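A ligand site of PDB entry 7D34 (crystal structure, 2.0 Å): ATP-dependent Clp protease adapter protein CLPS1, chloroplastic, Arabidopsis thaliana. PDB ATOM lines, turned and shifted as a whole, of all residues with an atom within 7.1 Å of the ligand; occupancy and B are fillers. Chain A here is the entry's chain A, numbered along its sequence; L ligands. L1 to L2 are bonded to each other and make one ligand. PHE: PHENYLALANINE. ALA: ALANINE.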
ATOM      1  N   LEU A   9      -3.315  11.839 -13.546  1.00  0.00           N
ATOM      2  CA  LEU A   9      -3.135  11.833 -12.100  1.00  0.00           C
ATOM      3  C   LEU A   9      -2.683  10.428 -11.711  1.00  0.00           C
ATOM      4  O   LEU A   9      -3.364   9.443 -12.039  1.00  0.00           O
ATOM      5  CB  LEU A   9      -4.429  12.223 -11.379  1.00  0.00           C
ATOM      6  CG  LEU A   9      -4.360  12.063  -9.858  1.00  0.00           C
ATOM      7  CD1 LEU A   9      -3.301  12.981  -9.236  1.00  0.00           C
ATOM      8  CD2 LEU A   9      -5.708  12.272  -9.216  1.00  0.00           C
ATOM      9  N   HIS A  10      -1.530  10.326 -11.070  1.00  0.00           N
ATOM     10  CA  HIS A  10      -1.012   9.053 -10.576  1.00  0.00           C
ATOM     11  C   HIS A  10      -1.251   8.912  -9.080  1.00  0.00           C
ATOM     12  O   HIS A  10      -1.193   9.890  -8.320  1.00  0.00           O
ATOM     13  CB  HIS A  10       0.482   8.952 -10.870  1.00  0.00           C
ATOM     14  CG  HIS A  10       0.833   8.990 -12.335  1.00  0.00           C
ATOM     15  ND1 HIS A  10       1.098   7.852 -13.061  1.00  0.00           N
ATOM     16  CD2 HIS A  10       0.973  10.031 -13.189  1.00  0.00           C
ATOM     17  CE1 HIS A  10       1.398   8.189 -14.301  1.00  0.00           C
ATOM     18  NE2 HIS A  10       1.326   9.498 -14.414  1.00  0.00           N
ATOM     19  N   ASN A  11      -1.519   7.676  -8.654  1.00  0.00           N
ATOM     20  CA  ASN A  11      -1.617   7.378  -7.230  1.00  0.00           C
ATOM     21  C   ASN A  11      -0.274   7.621  -6.538  1.00  0.00           C
ATOM     22  O   ASN A  11       0.797   7.413  -7.117  1.00  0.00           O
ATOM     23  CB  ASN A  11      -2.098   5.957  -7.014  1.00  0.00           C
ATOM     24  CG  ASN A  11      -2.553   5.713  -5.608  1.00  0.00           C
ATOM     25  OD1 ASN A  11      -3.373   6.440  -5.062  1.00  0.00           O
ATOM     26  ND2 ASN A  11      -2.041   4.665  -4.996  1.00  0.00           N
ATOM     27  N   ASP A  12      -0.352   8.092  -5.298  1.00  0.00           N
ATOM     28  CA  ASP A  12       0.803   8.255  -4.422  1.00  0.00           C
ATOM     29  C   ASP A  12       0.357   7.819  -3.021  1.00  0.00           C
ATOM     30  O   ASP A  12      -0.838   7.748  -2.739  1.00  0.00           O
ATOM     31  CB  ASP A  12       1.335   9.701  -4.449  1.00  0.00           C
ATOM     32  CG  ASP A  12       0.448  10.668  -3.714  1.00  0.00           C
ATOM     33  OD1 ASP A  12       0.344  10.550  -2.494  1.00  0.00           O
ATOM     34  OD2 ASP A  12      -0.158  11.548  -4.371  1.00  0.00           O
ATOM     35  N   ASN A  13       1.330   7.521  -2.161  1.00  0.00           N
ATOM     36  CA  ASN A  13       1.081   7.024  -0.807  1.00  0.00           C
ATOM     37  C   ASN A  13       1.302   8.101   0.260  1.00  0.00           C
ATOM     38  O   ASN A  13       1.668   7.783   1.392  1.00  0.00           O
ATOM     39  CB  ASN A  13       1.953   5.798  -0.498  1.00  0.00           C
ATOM     40  CG  ASN A  13       1.843   4.722  -1.554  1.00  0.00           C
ATOM     41  OD1 ASN A  13       0.751   4.433  -2.026  1.00  0.00           O
ATOM     42  ND2 ASN A  13       2.969   4.104  -1.909  1.00  0.00           N
ATOM     43  N   PHE A  14       1.095   9.357  -0.090  1.00  0.00           N
ATOM     44  CA  PHE A  14       1.304  10.465   0.830  1.00  0.00           C
ATOM     45  C   PHE A  14       0.073  11.328   1.019  1.00  0.00           C
ATOM     46  O   PHE A  14      -0.236  11.729   2.149  1.00  0.00           O
ATOM     47  CB  PHE A  14       2.471  11.347   0.335  1.00  0.00           C
ATOM     48  CG  PHE A  14       3.784  10.631   0.319  1.00  0.00           C
ATOM     49  CD1 PHE A  14       4.602  10.661   1.444  1.00  0.00           C
ATOM     50  CD2 PHE A  14       4.191   9.916  -0.779  1.00  0.00           C
ATOM     51  CE1 PHE A  14       5.811   9.988   1.444  1.00  0.00           C
ATOM     52  CE2 PHE A  14       5.393   9.250  -0.783  1.00  0.00           C
ATOM     53  CZ  PHE A  14       6.194   9.284   0.327  1.00  0.00           C
ATOM     54  N   ASN A  15      -0.643  11.662  -0.055  1.00  0.00           N
ATOM     55  CA  ASN A  15      -1.780  12.555   0.007  1.00  0.00           C
ATOM     56  C   ASN A  15      -3.039  11.852   0.476  1.00  0.00           C
ATOM     57  O   ASN A  15      -3.285  10.676   0.177  1.00  0.00           O
ATOM     58  CB  ASN A  15      -2.024  13.166  -1.372  1.00  0.00           C
ATOM     59  CG  ASN A  15      -0.924  14.118  -1.778  1.00  0.00           C
ATOM     60  OD1 ASN A  15      -0.715  15.166  -1.156  1.00  0.00           O
ATOM     61  ND2 ASN A  15      -0.176  13.719  -2.800  1.00  0.00           N
ATOM     62  N   LYS A  16      -3.877  12.598   1.194  1.00  0.00           N
ATOM     63  CA  LYS A  16      -5.125  12.067   1.707  1.00  0.00           C
ATOM     64  C   LYS A  16      -6.196  12.167   0.625  1.00  0.00           C
ATOM     65  O   LYS A  16      -6.159  13.064  -0.223  1.00  0.00           O
ATOM     66  CB  LYS A  16      -5.574  12.848   2.941  1.00  0.00           C
ATOM     67  CG  LYS A  16      -4.592  12.865   4.117  1.00  0.00           C
ATOM     68  CD  LYS A  16      -3.290  13.634   3.838  1.00  0.00           C
ATOM     69  CE  LYS A  16      -3.487  15.125   3.451  1.00  0.00           C
ATOM     70  NZ  LYS A  16      -2.344  15.560   2.640  1.00  0.00           N
ATOM     71  N   ARG A  17      -7.157  11.235   0.653  1.00  0.00           N
ATOM     72  CA  ARG A  17      -8.179  11.249  -0.393  1.00  0.00           C
ATOM     73  C   ARG A  17      -8.840  12.616  -0.503  1.00  0.00           C
ATOM     74  O   ARG A  17      -9.015  13.129  -1.612  1.00  0.00           O
ATOM     75  CB  ARG A  17      -9.244  10.180  -0.138  1.00  0.00           C
ATOM     76  CG  ARG A  17      -8.715   8.745  -0.057  1.00  0.00           C
ATOM     77  CD  ARG A  17      -9.800   7.854   0.530  1.00  0.00           C
ATOM     78  NE  ARG A  17     -10.765   7.483  -0.520  1.00  0.00           N
ATOM     79  CZ  ARG A  17     -10.510   6.626  -1.510  1.00  0.00           C
ATOM     80  NH1 ARG A  17     -11.452   6.383  -2.412  1.00  0.00           N
ATOM     81  NH2 ARG A  17      -9.319   6.054  -1.596  1.00  0.00           N
ATOM     82  N   GLU A  18      -9.184  13.234   0.615  1.00  0.00           N
ATOM     83  CA  GLU A  18      -9.897  14.502   0.586  1.00  0.00           C
ATOM     84  C   GLU A  18      -9.009  15.606   0.026  1.00  0.00           C
ATOM     85  O   GLU A  18      -9.475  16.466  -0.716  1.00  0.00           O
ATOM     86  CB  GLU A  18     -10.408  14.926   1.974  1.00  0.00           C
ATOM     87  CG  GLU A  18     -11.190  16.248   1.874  1.00  0.00           C
ATOM     88  CD  GLU A  18     -11.742  16.752   3.206  1.00  0.00           C
ATOM     89  OE1 GLU A  18     -11.229  16.314   4.264  1.00  0.00           O
ATOM     90  OE2 GLU A  18     -12.706  17.545   3.180  1.00  0.00           O
ATOM     91  N   VAL A  20      -6.534  15.252  -2.205  1.00  0.00           N
ATOM     92  CA  VAL A  20      -6.500  15.033  -3.652  1.00  0.00           C
ATOM     93  C   VAL A  20      -7.707  15.695  -4.305  1.00  0.00           C
ATOM     94  O   VAL A  20      -7.588  16.412  -5.304  1.00  0.00           O
ATOM     95  CB  VAL A  20      -6.444  13.528  -3.981  1.00  0.00           C
ATOM     96  CG1 VAL A  20      -6.530  13.309  -5.474  1.00  0.00           C
ATOM     97  CG2 VAL A  20      -5.196  12.828  -3.447  1.00  0.00           C
ATOM     98  N   ILE A  39     -12.107  10.885 -10.153  1.00  0.00           N
ATOM     99  CA  ILE A  39     -10.712  10.856 -10.565  1.00  0.00           C
ATOM    100  C   ILE A  39      -9.838  10.321  -9.442  1.00  0.00           C
ATOM    101  O   ILE A  39      -9.000   9.447  -9.638  1.00  0.00           O
ATOM    102  CB  ILE A  39     -10.269  12.266 -11.022  1.00  0.00           C
ATOM    103  CG1 ILE A  39     -11.120  12.744 -12.216  1.00  0.00           C
ATOM    104  CG2 ILE A  39      -8.798  12.289 -11.479  1.00  0.00           C
ATOM    105  CD1 ILE A  39     -10.902  14.175 -12.708  1.00  0.00           C
ATOM    106  N   MET A  40      -9.998  10.871  -8.240  1.00  0.00           N
ATOM    107  CA  MET A  40      -9.256  10.345  -7.105  1.00  0.00           C
ATOM    108  C   MET A  40      -9.491   8.842  -6.900  1.00  0.00           C
ATOM    109  O   MET A  40      -8.538   8.064  -6.764  1.00  0.00           O
ATOM    110  CB  MET A  40      -9.645  11.159  -5.893  1.00  0.00           C
ATOM    111  CG  MET A  40      -8.982  10.657  -4.648  1.00  0.00           C
ATOM    112  SD  MET A  40      -9.754   9.317  -3.714  1.00  0.00           S
ATOM    113  CE  MET A  40     -11.316  10.019  -3.278  1.00  0.00           C
ATOM    114  N   GLN A  41     -10.773   8.405  -6.931  1.00  0.00           N
ATOM    115  CA  GLN A  41     -11.119   6.991  -6.799  1.00  0.00           C
ATOM    116  C   GLN A  41     -10.402   6.155  -7.854  1.00  0.00           C
ATOM    117  O   GLN A  41      -9.755   5.145  -7.542  1.00  0.00           O
ATOM    118  CB  GLN A  41     -12.638   6.836  -6.901  1.00  0.00           C
ATOM    119  CG  GLN A  41     -13.371   6.958  -5.544  1.00  0.00           C
ATOM    120  CD  GLN A  41     -14.843   7.195  -5.700  1.00  0.00           C
ATOM    121  OE1 GLN A  41     -15.373   7.156  -6.800  1.00  0.00           O
ATOM    122  NE2 GLN A  41     -15.529   7.480  -4.586  1.00  0.00           N
ATOM    123  N   GLU A  42     -10.419   6.611  -9.106  1.00  0.00           N
ATOM    124  CA  GLU A  42      -9.864   5.839 -10.214  1.00  0.00           C
ATOM    125  C   GLU A  42      -8.348   5.735 -10.125  1.00  0.00           C
ATOM    126  O   GLU A  42      -7.785   4.689 -10.436  1.00  0.00           O
ATOM    127  CB  GLU A  42     -10.254   6.513 -11.529  1.00  0.00           C
ATOM    128  CG  GLU A  42     -11.666   6.174 -11.945  1.00  0.00           C
ATOM    129  CD  GLU A  42     -11.959   4.644 -11.897  1.00  0.00           C
ATOM    130  OE1 GLU A  42     -11.533   3.912 -12.815  1.00  0.00           O
ATOM    131  OE2 GLU A  42     -12.655   4.190 -10.949  1.00  0.00           O
ATOM    132  N   ALA A  43      -7.663   6.806  -9.751  1.00  0.00           N
ATOM    133  CA  ALA A  43      -6.213   6.737  -9.580  1.00  0.00           C
ATOM    134  C   ALA A  43      -5.851   5.819  -8.427  1.00  0.00           C
ATOM    135  O   ALA A  43      -4.875   5.068  -8.500  1.00  0.00           O
ATOM    136  CB  ALA A  43      -5.632   8.132  -9.356  1.00  0.00           C
ATOM    137  N   HIS A  44      -6.641   5.861  -7.352  1.00  0.00           N
ATOM    138  CA  HIS A  44      -6.383   5.016  -6.190  1.00  0.00           C
ATOM    139  C   HIS A  44      -6.526   3.537  -6.519  1.00  0.00           C
ATOM    140  O   HIS A  44      -5.725   2.711  -6.072  1.00  0.00           O
ATOM    141  CB  HIS A  44      -7.350   5.404  -5.049  1.00  0.00           C
ATOM    142  CG  HIS A  44      -7.244   4.535  -3.845  1.00  0.00           C
ATOM    143  ND1 HIS A  44      -6.241   4.694  -2.898  1.00  0.00           N
ATOM    144  CD2 HIS A  44      -7.992   3.493  -3.419  1.00  0.00           C
ATOM    145  CE1 HIS A  44      -6.391   3.792  -1.947  1.00  0.00           C
ATOM    146  NE2 HIS A  44      -7.440   3.050  -2.240  1.00  0.00           N
ATOM    147  N   ILE A  45      -7.545   3.181  -7.297  1.00  0.00           N
ATOM    148  CA  ILE A  45      -7.806   1.787  -7.625  1.00  0.00           C
ATOM    149  C   ILE A  45      -6.930   1.296  -8.770  1.00  0.00           C
ATOM    150  O   ILE A  45      -6.455   0.161  -8.739  1.00  0.00           O
ATOM    151  CB  ILE A  45      -9.306   1.601  -7.965  1.00  0.00           C
ATOM    152  CG1 ILE A  45     -10.153   1.675  -6.685  1.00  0.00           C
ATOM    153  CG2 ILE A  45      -9.524   0.289  -8.713  1.00  0.00           C
ATOM    154  CD1 ILE A  45      -9.945   0.519  -5.767  1.00  0.00           C
ATOM    155  N   GLY A  47      -4.123   3.015 -10.169  1.00  0.00           N
ATOM    156  CA  GLY A  47      -2.784   3.560 -10.240  1.00  0.00           C
ATOM    157  C   GLY A  47      -2.669   4.874 -10.995  1.00  0.00           C
ATOM    158  O   GLY A  47      -1.692   5.598 -10.803  1.00  0.00           O
ATOM    159  N   LEU A  71       0.858  16.556  -5.895  1.00  0.00           N
ATOM    160  CA  LEU A  71       0.371  15.348  -6.566  1.00  0.00           C
ATOM    161  C   LEU A  71       1.360  14.883  -7.640  1.00  0.00           C
ATOM    162  O   LEU A  71       2.256  15.614  -8.060  1.00  0.00           O
ATOM    163  CB  LEU A  71      -1.007  15.564  -7.184  1.00  0.00           C
ATOM    164  CG  LEU A  71      -2.045  16.227  -6.267  1.00  0.00           C
ATOM    165  CD1 LEU A  71      -3.422  16.243  -6.936  1.00  0.00           C
ATOM    166  CD2 LEU A  71      -2.093  15.602  -4.893  1.00  0.00           C
ATOM    167  N   LEU A  72       1.218  13.608  -8.032  1.00  0.00           N
ATOM    168  CA  LEU A  72       2.000  13.024  -9.114  1.00  0.00           C
ATOM    169  C   LEU A  72       1.198  13.105 -10.412  1.00  0.00           C
ATOM    170  O   LEU A  72       0.077  12.578 -10.472  1.00  0.00           O
ATOM    171  CB  LEU A  72       2.363  11.569  -8.820  1.00  0.00           C
ATOM    172  CG  LEU A  72       3.256  11.330  -7.611  1.00  0.00           C
ATOM    173  CD1 LEU A  72       3.462   9.854  -7.382  1.00  0.00           C
ATOM    174  CD2 LEU A  72       4.597  11.997  -7.839  1.00  0.00           C
HETATM  175  N   PHE L   1      -3.718   6.544  -2.392  1.00  0.00           N
HETATM  176  CA  PHE L   1      -3.956   7.710  -1.483  1.00  0.00           C
HETATM  177  C   PHE L   1      -4.323   7.224  -0.067  1.00  0.00           C
HETATM  178  O   PHE L   1      -4.875   6.129   0.091  1.00  0.00           O
HETATM  179  CB  PHE L   1      -5.067   8.604  -2.051  1.00  0.00           C
HETATM  180  CG  PHE L   1      -4.834   9.029  -3.484  1.00  0.00           C
HETATM  181  CD1 PHE L   1      -3.682   9.722  -3.847  1.00  0.00           C
HETATM  182  CD2 PHE L   1      -5.774   8.746  -4.470  1.00  0.00           C
HETATM  183  CE1 PHE L   1      -3.470  10.117  -5.172  1.00  0.00           C
HETATM  184  CE2 PHE L   1      -5.575   9.146  -5.792  1.00  0.00           C
HETATM  185  CZ  PHE L   1      -4.416   9.825  -6.138  1.00  0.00           C
HETATM  186  N   ALA L   2      -4.031   8.050   0.930  1.00  0.00           N
HETATM  187  CA  ALA L   2      -4.220   7.685   2.333  1.00  0.00           C
HETATM  188  C   ALA L   2      -5.622   7.995   2.898  1.00  0.00           C
HETATM  189  O   ALA L   2      -6.358   8.845   2.379  1.00  0.00           O
HETATM  190  CB  ALA L   2      -3.156   8.386   3.201  1.00  0.00           C
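OD1 of Asn 11 is in hydrogen-bond range of N of PHE L1 (2.7 Å).
O of Asn 15 lies within hydrogen-bond range of N of ALA L2, 2.8 Å away.
O of ALA L2 lies within hydrogen-bond range of N of Arg 17, 3.1 Å away.
The backbone carbonyl oxygen of Asp 12 sits at hydrogen-bond distance from a nitrogen (N) of PHE L1 (3.1 Å).
ND1 of His 44 is in hydrogen-bond range of N of PHE L1.
O of Gly 47 sits at hydrogen-bond distance from N of Asn 11, at 3.0 Å.
The side-chain amide nitrogen (ND2) of Asn 15 lies within hydrogen-bond range of the side-chain carboxylate (OD2) of Asp 12.
SD of Met 40 lies close to NH1 of Arg 17 (3.6 Å).
The side-chain carboxylate (OD1) of Asp 12 lies within hydrogen-bond range of the backbone NH (N) of Phe 14 (2.8 Å).
The backbone carbonyl oxygen of Leu 72 lies within hydrogen-bond range of the backbone NH of His 10 (2.8 Å).
Merely in contact with the ligand: His 10 (3.9 Å), Lys 16 (3.5 Å), Val 20 (3.5 Å), Met 40 (3.3 Å) and Ala 43 (3.7 Å).
Hydrophobic or aromatic side chains that line the ligand: Val 20, Met 40, Ala 43 and His 44.
The nearest printed residue that does not touch the ligand is Leu 9 (4.1 Å).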
